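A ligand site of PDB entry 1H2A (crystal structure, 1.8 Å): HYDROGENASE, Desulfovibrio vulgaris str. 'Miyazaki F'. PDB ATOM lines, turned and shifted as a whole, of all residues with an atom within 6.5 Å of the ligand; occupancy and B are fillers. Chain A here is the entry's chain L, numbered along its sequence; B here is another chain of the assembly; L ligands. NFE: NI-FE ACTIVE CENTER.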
ATOM      1  N   GLU A  34      23.975 -27.115 -20.835  1.00  0.00           N
ATOM      2  CA  GLU A  34      24.418 -26.866 -22.197  1.00  0.00           C
ATOM      3  C   GLU A  34      25.148 -25.533 -22.133  1.00  0.00           C
ATOM      4  O   GLU A  34      24.683 -24.591 -21.492  1.00  0.00           O
ATOM      5  CB  GLU A  34      23.223 -26.750 -23.138  1.00  0.00           C
ATOM      6  CG  GLU A  34      23.605 -26.689 -24.624  1.00  0.00           C
ATOM      7  CD  GLU A  34      24.342 -25.415 -25.010  1.00  0.00           C
ATOM      8  OE1 GLU A  34      24.062 -24.353 -24.411  1.00  0.00           O
ATOM      9  OE2 GLU A  34      25.211 -25.469 -25.885  1.00  0.00           O
ATOM     10  N   THR A  80      21.641 -22.013 -32.895  1.00  0.00           N
ATOM     11  CA  THR A  80      21.852 -21.315 -31.634  1.00  0.00           C
ATOM     12  C   THR A  80      21.920 -22.432 -30.572  1.00  0.00           C
ATOM     13  O   THR A  80      22.462 -22.243 -29.465  1.00  0.00           O
ATOM     14  CB  THR A  80      20.613 -20.436 -31.310  1.00  0.00           C
ATOM     15  OG1 THR A  80      20.383 -19.506 -32.376  1.00  0.00           O
ATOM     16  CG2 THR A  80      20.758 -19.705 -30.003  1.00  0.00           C
ATOM     17  N   CYS A  81      21.331 -23.588 -30.885  1.00  0.00           N
ATOM     18  CA  CYS A  81      21.309 -24.698 -29.956  1.00  0.00           C
ATOM     19  C   CYS A  81      20.962 -26.064 -30.540  1.00  0.00           C
ATOM     20  O   CYS A  81      20.218 -26.171 -31.551  1.00  0.00           O
ATOM     21  CB  CYS A  81      20.370 -24.383 -28.820  1.00  0.00           C
ATOM     22  SG  CYS A  81      20.661 -25.567 -27.477  1.00  0.00           S
ATOM     23  N   GLY A  82      21.522 -27.123 -29.940  1.00  0.00           N
ATOM     24  CA  GLY A  82      21.269 -28.471 -30.419  1.00  0.00           C
ATOM     25  C   GLY A  82      20.541 -29.310 -29.367  1.00  0.00           C
ATOM     26  O   GLY A  82      20.042 -30.380 -29.638  1.00  0.00           O
ATOM     27  N   VAL A  83      20.508 -28.810 -28.151  1.00  0.00           N
ATOM     28  CA  VAL A  83      19.818 -29.525 -27.088  1.00  0.00           C
ATOM     29  C   VAL A  83      18.338 -29.297 -27.384  1.00  0.00           C
ATOM     30  O   VAL A  83      17.639 -30.226 -27.716  1.00  0.00           O
ATOM     31  CB  VAL A  83      20.293 -29.032 -25.712  1.00  0.00           C
ATOM     32  CG1 VAL A  83      19.348 -29.424 -24.590  1.00  0.00           C
ATOM     33  CG2 VAL A  83      21.679 -29.622 -25.476  1.00  0.00           C
ATOM     34  N   CYS A  84      17.924 -28.033 -27.402  1.00  0.00           N
ATOM     35  CA  CYS A  84      16.539 -27.666 -27.705  1.00  0.00           C
ATOM     36  C   CYS A  84      16.558 -27.399 -29.210  1.00  0.00           C
ATOM     37  O   CYS A  84      16.276 -26.297 -29.692  1.00  0.00           O
ATOM     38  CB  CYS A  84      16.185 -26.396 -26.936  1.00  0.00           C
ATOM     39  SG  CYS A  84      17.213 -24.969 -27.406  1.00  0.00           S
ATOM     40  N   THR A  85      16.844 -28.447 -29.968  1.00  0.00           N
ATOM     41  CA  THR A  85      16.990 -28.352 -31.399  1.00  0.00           C
ATOM     42  C   THR A  85      15.950 -27.733 -32.311  1.00  0.00           C
ATOM     43  O   THR A  85      16.305 -26.906 -33.150  1.00  0.00           O
ATOM     44  CB  THR A  85      17.473 -29.665 -32.021  1.00  0.00           C
ATOM     45  OG1 THR A  85      17.645 -29.485 -33.429  1.00  0.00           O
ATOM     46  CG2 THR A  85      16.484 -30.827 -31.755  1.00  0.00           C
ATOM     47  N   THR A  87      13.062 -25.813 -31.599  1.00  0.00           N
ATOM     48  CA  THR A  87      12.525 -24.562 -31.138  1.00  0.00           C
ATOM     49  C   THR A  87      12.907 -23.282 -31.864  1.00  0.00           C
ATOM     50  O   THR A  87      12.028 -22.469 -32.169  1.00  0.00           O
ATOM     51  CB  THR A  87      12.829 -24.404 -29.664  1.00  0.00           C
ATOM     52  OG1 THR A  87      14.245 -24.248 -29.522  1.00  0.00           O
ATOM     53  CG2 THR A  87      12.377 -25.654 -28.905  1.00  0.00           C
ATOM     54  N   HIS A  88      14.201 -23.066 -32.107  1.00  0.00           N
ATOM     55  CA  HIS A  88      14.657 -21.836 -32.787  1.00  0.00           C
ATOM     56  C   HIS A  88      14.228 -21.782 -34.249  1.00  0.00           C
ATOM     57  O   HIS A  88      13.956 -20.703 -34.763  1.00  0.00           O
ATOM     58  CB  HIS A  88      16.188 -21.627 -32.687  1.00  0.00           C
ATOM     59  CG  HIS A  88      16.643 -21.159 -31.338  1.00  0.00           C
ATOM     60  ND1 HIS A  88      16.437 -19.875 -30.890  1.00  0.00           N
ATOM     61  CD2 HIS A  88      17.227 -21.830 -30.313  1.00  0.00           C
ATOM     62  CE1 HIS A  88      16.862 -19.771 -29.643  1.00  0.00           C
ATOM     63  NE2 HIS A  88      17.350 -20.936 -29.268  1.00  0.00           N
ATOM     64  N   GLN A 119       9.379 -32.984 -28.818  1.00  0.00           N
ATOM     65  CA  GLN A 119      10.634 -32.368 -28.347  1.00  0.00           C
ATOM     66  C   GLN A 119      10.571 -32.110 -26.865  1.00  0.00           C
ATOM     67  O   GLN A 119      11.589 -32.200 -26.187  1.00  0.00           O
ATOM     68  CB  GLN A 119      10.960 -31.062 -29.108  1.00  0.00           C
ATOM     69  CG  GLN A 119      11.935 -30.074 -28.404  1.00  0.00           C
ATOM     70  CD  GLN A 119      13.367 -30.557 -28.320  1.00  0.00           C
ATOM     71  OE1 GLN A 119      13.837 -31.285 -29.189  1.00  0.00           O
ATOM     72  NE2 GLN A 119      14.077 -30.146 -27.271  1.00  0.00           N
ATOM     73  N   ASP A 123      13.386 -33.882 -24.587  1.00  0.00           N
ATOM     74  CA  ASP A 123      14.138 -32.896 -23.798  1.00  0.00           C
ATOM     75  C   ASP A 123      14.038 -33.132 -22.303  1.00  0.00           C
ATOM     76  O   ASP A 123      15.046 -33.248 -21.609  1.00  0.00           O
ATOM     77  CB  ASP A 123      13.667 -31.462 -24.120  1.00  0.00           C
ATOM     78  CG  ASP A 123      14.770 -30.403 -23.961  1.00  0.00           C
ATOM     79  OD1 ASP A 123      15.623 -30.522 -23.047  1.00  0.00           O
ATOM     80  OD2 ASP A 123      14.750 -29.417 -24.738  1.00  0.00           O
ATOM     81  N   ALA A 477       9.137 -22.888 -25.333  1.00  0.00           N
ATOM     82  CA  ALA A 477       9.976 -24.067 -25.436  1.00  0.00           C
ATOM     83  C   ALA A 477      10.100 -24.757 -24.067  1.00  0.00           C
ATOM     84  O   ALA A 477       9.663 -24.210 -23.045  1.00  0.00           O
ATOM     85  CB  ALA A 477      11.354 -23.649 -25.938  1.00  0.00           C
ATOM     86  N   PRO A 478      10.773 -25.932 -24.008  1.00  0.00           N
ATOM     87  CA  PRO A 478      10.969 -26.697 -22.767  1.00  0.00           C
ATOM     88  C   PRO A 478      11.480 -25.840 -21.617  1.00  0.00           C
ATOM     89  O   PRO A 478      11.258 -26.169 -20.459  1.00  0.00           O
ATOM     90  CB  PRO A 478      12.016 -27.708 -23.169  1.00  0.00           C
ATOM     91  CG  PRO A 478      11.586 -28.063 -24.553  1.00  0.00           C
ATOM     92  CD  PRO A 478      11.244 -26.709 -25.172  1.00  0.00           C
ATOM     93  N   ARG A 479      12.221 -24.770 -21.943  1.00  0.00           N
ATOM     94  CA  ARG A 479      12.772 -23.871 -20.924  1.00  0.00           C
ATOM     95  C   ARG A 479      12.001 -22.563 -20.753  1.00  0.00           C
ATOM     96  O   ARG A 479      12.318 -21.744 -19.888  1.00  0.00           O
ATOM     97  CB  ARG A 479      14.241 -23.589 -21.251  1.00  0.00           C
ATOM     98  CG  ARG A 479      15.187 -24.687 -20.784  1.00  0.00           C
ATOM     99  CD  ARG A 479      16.447 -24.743 -21.591  1.00  0.00           C
ATOM    100  NE  ARG A 479      17.100 -26.033 -21.406  1.00  0.00           N
ATOM    101  CZ  ARG A 479      16.865 -27.123 -22.140  1.00  0.00           C
ATOM    102  NH1 ARG A 479      15.993 -27.115 -23.146  1.00  0.00           N
ATOM    103  NH2 ARG A 479      17.459 -28.250 -21.824  1.00  0.00           N
ATOM    104  N   GLY A 480      11.027 -22.313 -21.621  1.00  0.00           N
ATOM    105  CA  GLY A 480      10.245 -21.103 -21.446  1.00  0.00           C
ATOM    106  C   GLY A 480      10.006 -20.247 -22.653  1.00  0.00           C
ATOM    107  O   GLY A 480      10.170 -20.691 -23.792  1.00  0.00           O
ATOM    108  N   GLY A 481       9.609 -19.002 -22.373  1.00  0.00           N
ATOM    109  CA  GLY A 481       9.269 -18.015 -23.387  1.00  0.00           C
ATOM    110  C   GLY A 481      10.369 -17.611 -24.344  1.00  0.00           C
ATOM    111  O   GLY A 481      11.251 -16.818 -23.998  1.00  0.00           O
ATOM    112  N   LEU A 482      10.235 -18.085 -25.578  1.00  0.00           N
ATOM    113  CA  LEU A 482      11.163 -17.809 -26.660  1.00  0.00           C
ATOM    114  C   LEU A 482      10.555 -16.847 -27.712  1.00  0.00           C
ATOM    115  O   LEU A 482       9.418 -17.048 -28.142  1.00  0.00           O
ATOM    116  CB  LEU A 482      11.548 -19.115 -27.343  1.00  0.00           C
ATOM    117  CG  LEU A 482      12.411 -18.917 -28.579  1.00  0.00           C
ATOM    118  CD1 LEU A 482      13.688 -18.136 -28.180  1.00  0.00           C
ATOM    119  CD2 LEU A 482      12.753 -20.256 -29.201  1.00  0.00           C
ATOM    120  N   VAL A 500      15.874 -15.259 -25.663  1.00  0.00           N
ATOM    121  CA  VAL A 500      15.581 -16.649 -25.275  1.00  0.00           C
ATOM    122  C   VAL A 500      15.322 -16.916 -23.794  1.00  0.00           C
ATOM    123  O   VAL A 500      15.637 -16.086 -22.937  1.00  0.00           O
ATOM    124  CB  VAL A 500      16.670 -17.600 -25.796  1.00  0.00           C
ATOM    125  CG1 VAL A 500      17.236 -17.095 -27.102  1.00  0.00           C
ATOM    126  CG2 VAL A 500      17.769 -17.755 -24.755  1.00  0.00           C
ATOM    127  N   PRO A 501      14.715 -18.074 -23.464  1.00  0.00           N
ATOM    128  CA  PRO A 501      14.413 -18.446 -22.073  1.00  0.00           C
ATOM    129  C   PRO A 501      15.553 -18.281 -21.059  1.00  0.00           C
ATOM    130  O   PRO A 501      15.378 -17.652 -20.004  1.00  0.00           O
ATOM    131  CB  PRO A 501      13.971 -19.896 -22.194  1.00  0.00           C
ATOM    132  CG  PRO A 501      13.314 -19.945 -23.537  1.00  0.00           C
ATOM    133  CD  PRO A 501      14.237 -19.112 -24.399  1.00  0.00           C
ATOM    134  N   SER A 502      16.732 -18.835 -21.368  1.00  0.00           N
ATOM    135  CA  SER A 502      17.835 -18.724 -20.415  1.00  0.00           C
ATOM    136  C   SER A 502      18.333 -17.309 -20.189  1.00  0.00           C
ATOM    137  O   SER A 502      18.884 -17.005 -19.111  1.00  0.00           O
ATOM    138  CB  SER A 502      18.965 -19.675 -20.784  1.00  0.00           C
ATOM    139  OG  SER A 502      18.456 -20.987 -20.898  1.00  0.00           O
ATOM    140  N   THR A 503      18.081 -16.422 -21.155  1.00  0.00           N
ATOM    141  CA  THR A 503      18.479 -15.031 -21.030  1.00  0.00           C
ATOM    142  C   THR A 503      17.632 -14.493 -19.873  1.00  0.00           C
ATOM    143  O   THR A 503      18.139 -13.814 -18.989  1.00  0.00           O
ATOM    144  CB  THR A 503      18.179 -14.218 -22.312  1.00  0.00           C
ATOM    145  OG1 THR A 503      18.420 -15.020 -23.477  1.00  0.00           O
ATOM    146  CG2 THR A 503      19.094 -13.026 -22.382  1.00  0.00           C
ATOM    147  N   THR A 505      16.125 -16.189 -17.265  1.00  0.00           N
ATOM    148  CA  THR A 505      16.500 -16.761 -15.980  1.00  0.00           C
ATOM    149  C   THR A 505      17.962 -16.720 -15.578  1.00  0.00           C
ATOM    150  O   THR A 505      18.267 -16.408 -14.429  1.00  0.00           O
ATOM    151  CB  THR A 505      16.005 -18.192 -15.865  1.00  0.00           C
ATOM    152  OG1 THR A 505      16.320 -18.886 -17.084  1.00  0.00           O
ATOM    153  CG2 THR A 505      14.521 -18.208 -15.658  1.00  0.00           C
ATOM    154  N   ASP A 544      17.535 -25.881 -15.603  1.00  0.00           N
ATOM    155  CA  ASP A 544      17.828 -26.489 -16.903  1.00  0.00           C
ATOM    156  C   ASP A 544      18.491 -25.398 -17.788  1.00  0.00           C
ATOM    157  O   ASP A 544      18.059 -25.139 -18.916  1.00  0.00           O
ATOM    158  CB  ASP A 544      16.470 -26.987 -17.465  1.00  0.00           C
ATOM    159  CG  ASP A 544      16.577 -27.798 -18.727  1.00  0.00           C
ATOM    160  OD1 ASP A 544      17.702 -28.167 -19.135  1.00  0.00           O
ATOM    161  OD2 ASP A 544      15.504 -28.073 -19.350  1.00  0.00           O
ATOM    162  N   PRO A 545      19.601 -24.790 -17.316  1.00  0.00           N
ATOM    163  CA  PRO A 545      20.265 -23.736 -18.111  1.00  0.00           C
ATOM    164  C   PRO A 545      20.882 -24.181 -19.418  1.00  0.00           C
ATOM    165  O   PRO A 545      21.404 -25.283 -19.508  1.00  0.00           O
ATOM    166  CB  PRO A 545      21.313 -23.150 -17.161  1.00  0.00           C
ATOM    167  CG  PRO A 545      21.650 -24.292 -16.277  1.00  0.00           C
ATOM    168  CD  PRO A 545      20.319 -24.996 -16.038  1.00  0.00           C
ATOM    169  N   CYS A 546      20.733 -23.328 -20.429  1.00  0.00           N
ATOM    170  CA  CYS A 546      21.277 -23.542 -21.771  1.00  0.00           C
ATOM    171  C   CYS A 546      21.979 -22.241 -22.186  1.00  0.00           C
ATOM    172  O   CYS A 546      21.332 -21.251 -22.560  1.00  0.00           O
ATOM    173  CB  CYS A 546      20.149 -23.857 -22.737  1.00  0.00           C
ATOM    174  SG  CYS A 546      20.720 -24.191 -24.427  1.00  0.00           S
ATOM    175  N   ILE A 547      23.320 -22.246 -22.105  1.00  0.00           N
ATOM    176  CA  ILE A 547      24.110 -21.048 -22.394  1.00  0.00           C
ATOM    177  C   ILE A 547      24.277 -20.608 -23.862  1.00  0.00           C
ATOM    178  O   ILE A 547      24.308 -19.404 -24.159  1.00  0.00           O
ATOM    179  CB  ILE A 547      25.473 -21.147 -21.680  1.00  0.00           C
ATOM    180  CG1 ILE A 547      25.238 -21.600 -20.236  1.00  0.00           C
ATOM    181  CG2 ILE A 547      26.174 -19.800 -21.660  1.00  0.00           C
ATOM    182  CD1 ILE A 547      24.398 -20.644 -19.440  1.00  0.00           C
ATOM    183  N   ALA A 548      24.404 -21.550 -24.771  1.00  0.00           N
ATOM    184  CA  ALA A 548      24.521 -21.228 -26.170  1.00  0.00           C
ATOM    185  C   ALA A 548      23.194 -20.553 -26.614  1.00  0.00           C
ATOM    186  O   ALA A 548      23.194 -19.655 -27.486  1.00  0.00           O
ATOM    187  CB  ALA A 548      24.823 -22.448 -26.979  1.00  0.00           C
ATOM    188  N   CYS A 549      22.082 -20.930 -25.959  1.00  0.00           N
ATOM    189  CA  CYS A 549      20.788 -20.324 -26.267  1.00  0.00           C
ATOM    190  C   CYS A 549      20.794 -18.897 -25.742  1.00  0.00           C
ATOM    191  O   CYS A 549      20.595 -17.964 -26.497  1.00  0.00           O
ATOM    192  CB  CYS A 549      19.597 -21.093 -25.596  1.00  0.00           C
ATOM    193  SG  CYS A 549      18.784 -22.333 -26.677  1.00  0.00           S
ATOM    194  N   GLY A 550      21.085 -18.726 -24.458  1.00  0.00           N
ATOM    195  CA  GLY A 550      21.066 -17.403 -23.853  1.00  0.00           C
ATOM    196  C   GLY A 550      21.926 -16.275 -24.401  1.00  0.00           C
ATOM    197  O   GLY A 550      21.613 -15.106 -24.168  1.00  0.00           O
ATOM    198  N   CYS B  67      26.947 -25.331 -30.236  1.00  0.00           N
ATOM    199  CA  CYS B  67      25.536 -25.373 -29.823  1.00  0.00           C
ATOM    200  C   CYS B  67      25.170 -26.725 -29.193  1.00  0.00           C
ATOM    201  O   CYS B  67      23.991 -26.987 -28.945  1.00  0.00           O
ATOM    202  CB  CYS B  67      24.599 -25.146 -31.044  1.00  0.00           C
ATOM    203  SG  CYS B  67      24.599 -26.522 -32.275  1.00  0.00           S
HETATM  204 NI   NFE L   1      19.183 -24.597 -26.137  1.00  0.00          NI
HETATM  205 FE   NFE L   1      16.893 -23.510 -25.875  1.00  0.00          FE
HETATM  206  C1  NFE L   1      15.846 -22.274 -26.700  1.00  0.00           C
HETATM  207  C2  NFE L   1      15.226 -24.270 -25.254  1.00  0.00           C
HETATM  208  S3  NFE L   1      16.686 -22.185 -24.240  1.00  0.00           S
HETATM  209  S4  NFE L   1      18.137 -24.382 -24.252  1.00  0.00           S
HETATM  210  O1  NFE L   1      15.131 -21.292 -26.696  1.00  0.00           O
HETATM  211  O2  NFE L   1      14.324 -24.430 -24.425  1.00  0.00           O
HETATM  212  O3  NFE L   1      16.859 -21.285 -22.931  1.00  0.00           O
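An iron atom (FE) of the ligand is bound by the side-chain sulfur (SG) of Cys 84 (2.1 Å). NI of the ligand is bound by SG of Cys 81 (2.2 Å). NI of the ligand is bound by SG of Cys 546, at 2.3 Å. The side-chain sulfur of Cys 549 binds a nickel atom (NI) of the ligand (2.4 Å). The backbone NH of Ser 502 lies within hydrogen-bond range of an oxygen (O3) of the ligand (2.9 Å). OG of Ser 502 sits at hydrogen-bond distance from O3 of the ligand. An oxygen (O2) of the ligand is in hydrogen-bond range of the backbone NH of Arg 479 (3.3 Å). The guanidinium group (NH1) of Arg 479 sits close to an oxygen (O2) of the ligand. An oxygen (O1) of the ligand lies close to a ring nitrogen (NE2) of His 88, 3.4 Å away.
O of Cys 84 sits at hydrogen-bond distance from OG1 of Thr 87. The side-chain sulfur (SG) of Cys 81 sits close to the backbone NH (N) of Val 83 (3.3 Å). The backbone NH of Cys 546 lies within hydrogen-bond range of the side-chain hydroxyl of Ser 502, at 3.3 Å. SG of Cys 546 lies close to OE1 of Glu 34 (3.3 Å). SG of Cys 549 lies close to NE2 of His 88 (3.3 Å). The side-chain carboxylate of Asp 123 lies within salt-bridge range of the guanidinium group of Arg 479 (3.1 Å). NH2 of Arg 479 is in salt-bridge range of OD1 of Asp 544. The backbone carbonyl oxygen (O) of Pro 501 sits at hydrogen-bond distance from the side-chain hydroxyl (OG1) of Thr 505, 3.3 Å away.
Thr 87 touches the ligand (OG1 to C1, 3.8 Å). Ala 477 touches the ligand (CB to O2, 3.4 Å). N of Pro 478 touches O2 of the ligand, 3.9 Å away. Leu 482 touches the ligand. CB of Pro 501 touches O3 of the ligand, 3.3 Å away. Hydrophobic or aromatic side chains that line the ligand: His 88, Ala 477, Pro 478, Leu 482 and Pro 501.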
